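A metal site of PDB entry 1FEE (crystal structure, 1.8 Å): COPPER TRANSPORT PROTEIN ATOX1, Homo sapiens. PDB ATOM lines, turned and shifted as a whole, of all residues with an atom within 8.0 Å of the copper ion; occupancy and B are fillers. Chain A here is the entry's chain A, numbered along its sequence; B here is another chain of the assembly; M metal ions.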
ATOM      1  N   ASP A   9      11.565  -9.681  33.251  1.00  0.00           N
ATOM      2  CA  ASP A   9      11.505  -8.327  32.725  1.00  0.00           C
ATOM      3  C   ASP A   9      10.943  -8.275  31.297  1.00  0.00           C
ATOM      4  O   ASP A   9      11.684  -8.353  30.319  1.00  0.00           O
ATOM      5  CB  ASP A   9      12.887  -7.684  32.743  1.00  0.00           C
ATOM      6  CG  ASP A   9      12.821  -6.164  32.656  1.00  0.00           C
ATOM      7  OD1 ASP A   9      11.742  -5.635  32.338  1.00  0.00           O
ATOM      8  OD2 ASP A   9      13.858  -5.510  32.893  1.00  0.00           O
ATOM      9  N   MET A  10       9.615  -8.148  31.209  1.00  0.00           N
ATOM     10  CA  MET A  10       8.928  -8.066  29.926  1.00  0.00           C
ATOM     11  C   MET A  10       8.399  -6.646  29.826  1.00  0.00           C
ATOM     12  O   MET A  10       7.861  -6.110  30.795  1.00  0.00           O
ATOM     13  CB  MET A  10       7.754  -9.053  29.909  1.00  0.00           C
ATOM     14  CG  MET A  10       8.166 -10.479  30.244  1.00  0.00           C
ATOM     15  SD  MET A  10       6.767 -11.574  30.524  1.00  0.00           S
ATOM     16  CE  MET A  10       6.252 -11.049  32.151  1.00  0.00           C
ATOM     17  N   THR A  11       8.543  -6.018  28.653  1.00  0.00           N
ATOM     18  CA  THR A  11       8.083  -4.647  28.487  1.00  0.00           C
ATOM     19  C   THR A  11       7.127  -4.370  27.312  1.00  0.00           C
ATOM     20  O   THR A  11       6.885  -3.219  26.971  1.00  0.00           O
ATOM     21  CB  THR A  11       9.278  -3.667  28.398  1.00  0.00           C
ATOM     22  OG1 THR A  11      10.271  -4.210  27.522  1.00  0.00           O
ATOM     23  CG2 THR A  11       9.892  -3.457  29.776  1.00  0.00           C
ATOM     24  N   CYS A  12       6.613  -5.428  26.702  1.00  0.00           N
ATOM     25  CA  CYS A  12       5.652  -5.305  25.606  1.00  0.00           C
ATOM     26  C   CYS A  12       4.983  -6.663  25.419  1.00  0.00           C
ATOM     27  O   CYS A  12       5.456  -7.668  25.966  1.00  0.00           O
ATOM     28  CB  CYS A  12       6.321  -4.859  24.294  1.00  0.00           C
ATOM     29  SG  CYS A  12       7.158  -6.135  23.321  1.00  0.00           S
ATOM     30  N   GLY A  13       3.885  -6.705  24.675  1.00  0.00           N
ATOM     31  CA  GLY A  13       3.193  -7.955  24.436  1.00  0.00           C
ATOM     32  C   GLY A  13       4.082  -8.981  23.741  1.00  0.00           C
ATOM     33  O   GLY A  13       3.934 -10.183  23.941  1.00  0.00           O
ATOM     34  N   GLY A  14       4.996  -8.494  22.913  1.00  0.00           N
ATOM     35  CA  GLY A  14       5.905  -9.376  22.212  1.00  0.00           C
ATOM     36  C   GLY A  14       6.829 -10.071  23.197  1.00  0.00           C
ATOM     37  O   GLY A  14       7.215 -11.221  22.988  1.00  0.00           O
ATOM     38  N   CYS A  15       7.177  -9.369  24.269  1.00  0.00           N
ATOM     39  CA  CYS A  15       8.049  -9.941  25.308  1.00  0.00           C
ATOM     40  C   CYS A  15       7.327 -11.123  25.981  1.00  0.00           C
ATOM     41  O   CYS A  15       7.922 -12.158  26.238  1.00  0.00           O
ATOM     42  CB  CYS A  15       8.384  -8.884  26.374  1.00  0.00           C
ATOM     43  SG  CYS A  15       9.703  -7.692  25.945  1.00  0.00           S
ATOM     44  N   ALA A  16       6.037 -10.930  26.276  1.00  0.00           N
ATOM     45  CA  ALA A  16       5.241 -11.971  26.910  1.00  0.00           C
ATOM     46  C   ALA A  16       5.050 -13.153  25.962  1.00  0.00           C
ATOM     47  O   ALA A  16       5.102 -14.317  26.379  1.00  0.00           O
ATOM     48  CB  ALA A  16       3.892 -11.424  27.341  1.00  0.00           C
ATOM     49  N   GLU A  17       4.804 -12.850  24.695  1.00  0.00           N
ATOM     50  CA  GLU A  17       4.627 -13.888  23.689  1.00  0.00           C
ATOM     51  C   GLU A  17       5.877 -14.769  23.610  1.00  0.00           C
ATOM     52  O   GLU A  17       5.791 -15.990  23.473  1.00  0.00           O
ATOM     53  CB  GLU A  17       4.340 -13.242  22.330  1.00  0.00           C
ATOM     54  CG  GLU A  17       4.312 -14.207  21.163  1.00  0.00           C
ATOM     55  CD  GLU A  17       4.188 -13.495  19.821  1.00  0.00           C
ATOM     56  OE1 GLU A  17       5.012 -12.602  19.541  1.00  0.00           O
ATOM     57  OE2 GLU A  17       3.276 -13.838  19.049  1.00  0.00           O
ATOM     58  N   ALA A  18       7.047 -14.134  23.700  1.00  0.00           N
ATOM     59  CA  ALA A  18       8.311 -14.863  23.629  1.00  0.00           C
ATOM     60  C   ALA A  18       8.430 -15.842  24.793  1.00  0.00           C
ATOM     61  O   ALA A  18       8.880 -16.977  24.613  1.00  0.00           O
ATOM     62  CB  ALA A  18       9.485 -13.890  23.625  1.00  0.00           C
ATOM     63  N   LEU A  35       1.826  -9.092  32.367  1.00  0.00           N
ATOM     64  CA  LEU A  35       2.778  -8.137  31.793  1.00  0.00           C
ATOM     65  C   LEU A  35       3.063  -6.902  32.659  1.00  0.00           C
ATOM     66  O   LEU A  35       4.224  -6.592  32.943  1.00  0.00           O
ATOM     67  CB  LEU A  35       2.321  -7.712  30.386  1.00  0.00           C
ATOM     68  CG  LEU A  35       3.214  -6.698  29.671  1.00  0.00           C
ATOM     69  CD1 LEU A  35       4.646  -7.232  29.585  1.00  0.00           C
ATOM     70  CD2 LEU A  35       2.671  -6.423  28.270  1.00  0.00           C
ATOM     71  N   LYS A  60      16.196 -12.533  28.698  1.00  0.00           N
ATOM     72  CA  LYS A  60      15.512 -11.574  29.564  1.00  0.00           C
ATOM     73  C   LYS A  60      16.010 -11.712  30.993  1.00  0.00           C
ATOM     74  O   LYS A  60      16.533 -12.760  31.375  1.00  0.00           O
ATOM     75  CB  LYS A  60      13.999 -11.801  29.513  1.00  0.00           C
ATOM     76  CG  LYS A  60      13.413 -11.701  28.106  1.00  0.00           C
ATOM     77  CD  LYS A  60      11.881 -11.693  28.123  1.00  0.00           C
ATOM     78  CE  LYS A  60      11.313 -11.803  26.710  1.00  0.00           C
ATOM     79  NZ  LYS A  60      11.871 -10.773  25.790  1.00  0.00           N
ATOM     80  N   ASP B   9      11.495 -10.629  15.102  1.00  0.00           N
ATOM     81  CA  ASP B   9      10.299  -9.886  15.478  1.00  0.00           C
ATOM     82  C   ASP B   9      10.372  -9.209  16.853  1.00  0.00           C
ATOM     83  O   ASP B   9       9.736  -9.641  17.802  1.00  0.00           O
ATOM     84  CB  ASP B   9       9.092 -10.823  15.396  1.00  0.00           C
ATOM     85  CG  ASP B   9       7.789 -10.135  15.742  1.00  0.00           C
ATOM     86  OD1 ASP B   9       7.613  -8.969  15.334  1.00  0.00           O
ATOM     87  OD2 ASP B   9       6.941 -10.778  16.395  1.00  0.00           O
ATOM     88  N   MET B  10      11.154  -8.137  16.937  1.00  0.00           N
ATOM     89  CA  MET B  10      11.326  -7.373  18.166  1.00  0.00           C
ATOM     90  C   MET B  10      10.341  -6.204  18.136  1.00  0.00           C
ATOM     91  O   MET B  10      10.229  -5.522  17.115  1.00  0.00           O
ATOM     92  CB  MET B  10      12.750  -6.816  18.245  1.00  0.00           C
ATOM     93  CG  MET B  10      13.852  -7.831  18.066  1.00  0.00           C
ATOM     94  SD  MET B  10      15.466  -7.027  17.845  1.00  0.00           S
ATOM     95  CE  MET B  10      15.359  -6.536  16.085  1.00  0.00           C
ATOM     96  N   THR B  11       9.642  -5.954  19.237  1.00  0.00           N
ATOM     97  CA  THR B  11       8.687  -4.854  19.260  1.00  0.00           C
ATOM     98  C   THR B  11       8.905  -3.769  20.317  1.00  0.00           C
ATOM     99  O   THR B  11       8.110  -2.838  20.439  1.00  0.00           O
ATOM    100  CB  THR B  11       7.226  -5.381  19.330  1.00  0.00           C
ATOM    101  OG1 THR B  11       7.126  -6.382  20.352  1.00  0.00           O
ATOM    102  CG2 THR B  11       6.835  -6.004  18.003  1.00  0.00           C
ATOM    103  N   CYS B  12       9.975  -3.903  21.096  1.00  0.00           N
ATOM    104  CA  CYS B  12      10.316  -2.900  22.110  1.00  0.00           C
ATOM    105  C   CYS B  12      11.808  -2.955  22.411  1.00  0.00           C
ATOM    106  O   CYS B  12      12.493  -3.893  22.000  1.00  0.00           O
ATOM    107  CB  CYS B  12       9.493  -3.110  23.387  1.00  0.00           C
ATOM    108  SG  CYS B  12      10.175  -4.295  24.590  1.00  0.00           S
ATOM    109  N   GLY B  13      12.300  -1.959  23.134  1.00  0.00           N
ATOM    110  CA  GLY B  13      13.718  -1.920  23.489  1.00  0.00           C
ATOM    111  C   GLY B  13      14.145  -3.138  24.281  1.00  0.00           C
ATOM    112  O   GLY B  13      15.276  -3.614  24.132  1.00  0.00           O
ATOM    113  N   GLY B  14      13.247  -3.623  25.128  1.00  0.00           N
ATOM    114  CA  GLY B  14      13.541  -4.803  25.935  1.00  0.00           C
ATOM    115  C   GLY B  14      13.762  -6.013  25.054  1.00  0.00           C
ATOM    116  O   GLY B  14      14.555  -6.894  25.391  1.00  0.00           O
ATOM    117  N   CYS B  15      13.050  -6.070  23.923  1.00  0.00           N
ATOM    118  CA  CYS B  15      13.188  -7.161  22.964  1.00  0.00           C
ATOM    119  C   CYS B  15      14.606  -7.124  22.375  1.00  0.00           C
ATOM    120  O   CYS B  15      15.264  -8.151  22.227  1.00  0.00           O
ATOM    121  CB  CYS B  15      12.178  -7.028  21.811  1.00  0.00           C
ATOM    122  SG  CYS B  15      10.419  -7.362  22.206  1.00  0.00           S
ATOM    123  N   ALA B  16      15.059  -5.915  22.049  1.00  0.00           N
ATOM    124  CA  ALA B  16      16.392  -5.727  21.495  1.00  0.00           C
ATOM    125  C   ALA B  16      17.472  -6.099  22.511  1.00  0.00           C
ATOM    126  O   ALA B  16      18.479  -6.712  22.149  1.00  0.00           O
ATOM    127  CB  ALA B  16      16.573  -4.260  21.038  1.00  0.00           C
ATOM    128  N   GLU B  17      17.269  -5.726  23.768  1.00  0.00           N
ATOM    129  CA  GLU B  17      18.243  -6.060  24.808  1.00  0.00           C
ATOM    130  C   GLU B  17      18.390  -7.566  24.966  1.00  0.00           C
ATOM    131  O   GLU B  17      19.489  -8.081  25.154  1.00  0.00           O
ATOM    132  CB  GLU B  17      17.834  -5.437  26.155  1.00  0.00           C
ATOM    133  CG  GLU B  17      17.763  -3.920  26.148  1.00  0.00           C
ATOM    134  CD  GLU B  17      17.242  -3.359  27.459  1.00  0.00           C
ATOM    135  OE1 GLU B  17      16.468  -4.074  28.143  1.00  0.00           O
ATOM    136  OE2 GLU B  17      17.573  -2.206  27.803  1.00  0.00           O
ATOM    137  N   ALA B  18      17.267  -8.288  24.877  1.00  0.00           N
ATOM    138  CA  ALA B  18      17.285  -9.744  25.010  1.00  0.00           C
ATOM    139  C   ALA B  18      18.090 -10.370  23.883  1.00  0.00           C
ATOM    140  O   ALA B  18      18.864 -11.310  24.108  1.00  0.00           O
ATOM    141  CB  ALA B  18      15.853 -10.290  25.018  1.00  0.00           C
ATOM    142  N   LEU B  35      16.073  -2.125  15.551  1.00  0.00           N
ATOM    143  CA  LEU B  35      14.767  -2.366  16.143  1.00  0.00           C
ATOM    144  C   LEU B  35      13.568  -2.005  15.274  1.00  0.00           C
ATOM    145  O   LEU B  35      12.691  -2.846  15.029  1.00  0.00           O
ATOM    146  CB  LEU B  35      14.671  -1.661  17.505  1.00  0.00           C
ATOM    147  CG  LEU B  35      13.345  -1.702  18.265  1.00  0.00           C
ATOM    148  CD1 LEU B  35      12.904  -3.146  18.472  1.00  0.00           C
ATOM    149  CD2 LEU B  35      13.508  -0.999  19.612  1.00  0.00           C
ATOM    150  N   LYS B  60      11.443 -15.395  20.050  1.00  0.00           N
ATOM    151  CA  LYS B  60      10.877 -14.500  19.042  1.00  0.00           C
ATOM    152  C   LYS B  60      10.895 -15.193  17.686  1.00  0.00           C
ATOM    153  O   LYS B  60      11.655 -16.141  17.472  1.00  0.00           O
ATOM    154  CB  LYS B  60      11.692 -13.210  18.961  1.00  0.00           C
ATOM    155  CG  LYS B  60      11.741 -12.403  20.260  1.00  0.00           C
ATOM    156  CD  LYS B  60      12.638 -11.190  20.078  1.00  0.00           C
ATOM    157  CE  LYS B  60      12.706 -10.335  21.339  1.00  0.00           C
ATOM    158  NZ  LYS B  60      13.265 -11.076  22.504  1.00  0.00           N
HETATM  159 CU    CU M   1       9.342  -6.356  23.999  1.00  0.00          CU
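N of Gly 14 of chain A lies close to SG of Cys 12 of chain A (3.2 Å). The side-chain sulfur of Cys 15 of chain B sits close to the backbone NH of Thr 11 of chain B (3.4 Å). The side-chain sulfur (SG) of Cys 12 of chain B sits close to the backbone NH (N) of Gly 14 of chain B (3.2 Å). The side-chain sulfur (SG) of Cys 15 of chain A sits close to the side-chain amino group (NZ) of Lys 60 of chain A (3.8 Å). The side-chain sulfur (SG) of Cys 15 of chain A sits close to the backbone NH (N) of Thr 11 of chain A (3.4 Å). SG of Cys 12 of chain B lies close to OG1 of Thr 11 of chain A (2.9 Å). The side-chain sulfur (SG) of Cys 12 of chain A lies close to the side-chain hydroxyl (OG1) of Thr 11 of chain B.
The copper ion is bound by the side-chain sulfur (SG) of Cys 12 of chain A (2.3 Å), the side-chain sulfur (SG) of Cys 12 of chain B (2.3 Å), the side-chain sulfur (SG) of Cys 15 of chain B (2.3 Å) and the side-chain sulfur (SG) of Cys 15 of chain A (2.4 Å). The copper ion has four donor atoms within binding distance.
Within 4 Å of the copper ion: Cys 12 of chain A, Cys 15 of chain A, Cys 12 of chain B and Cys 15 of chain B.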
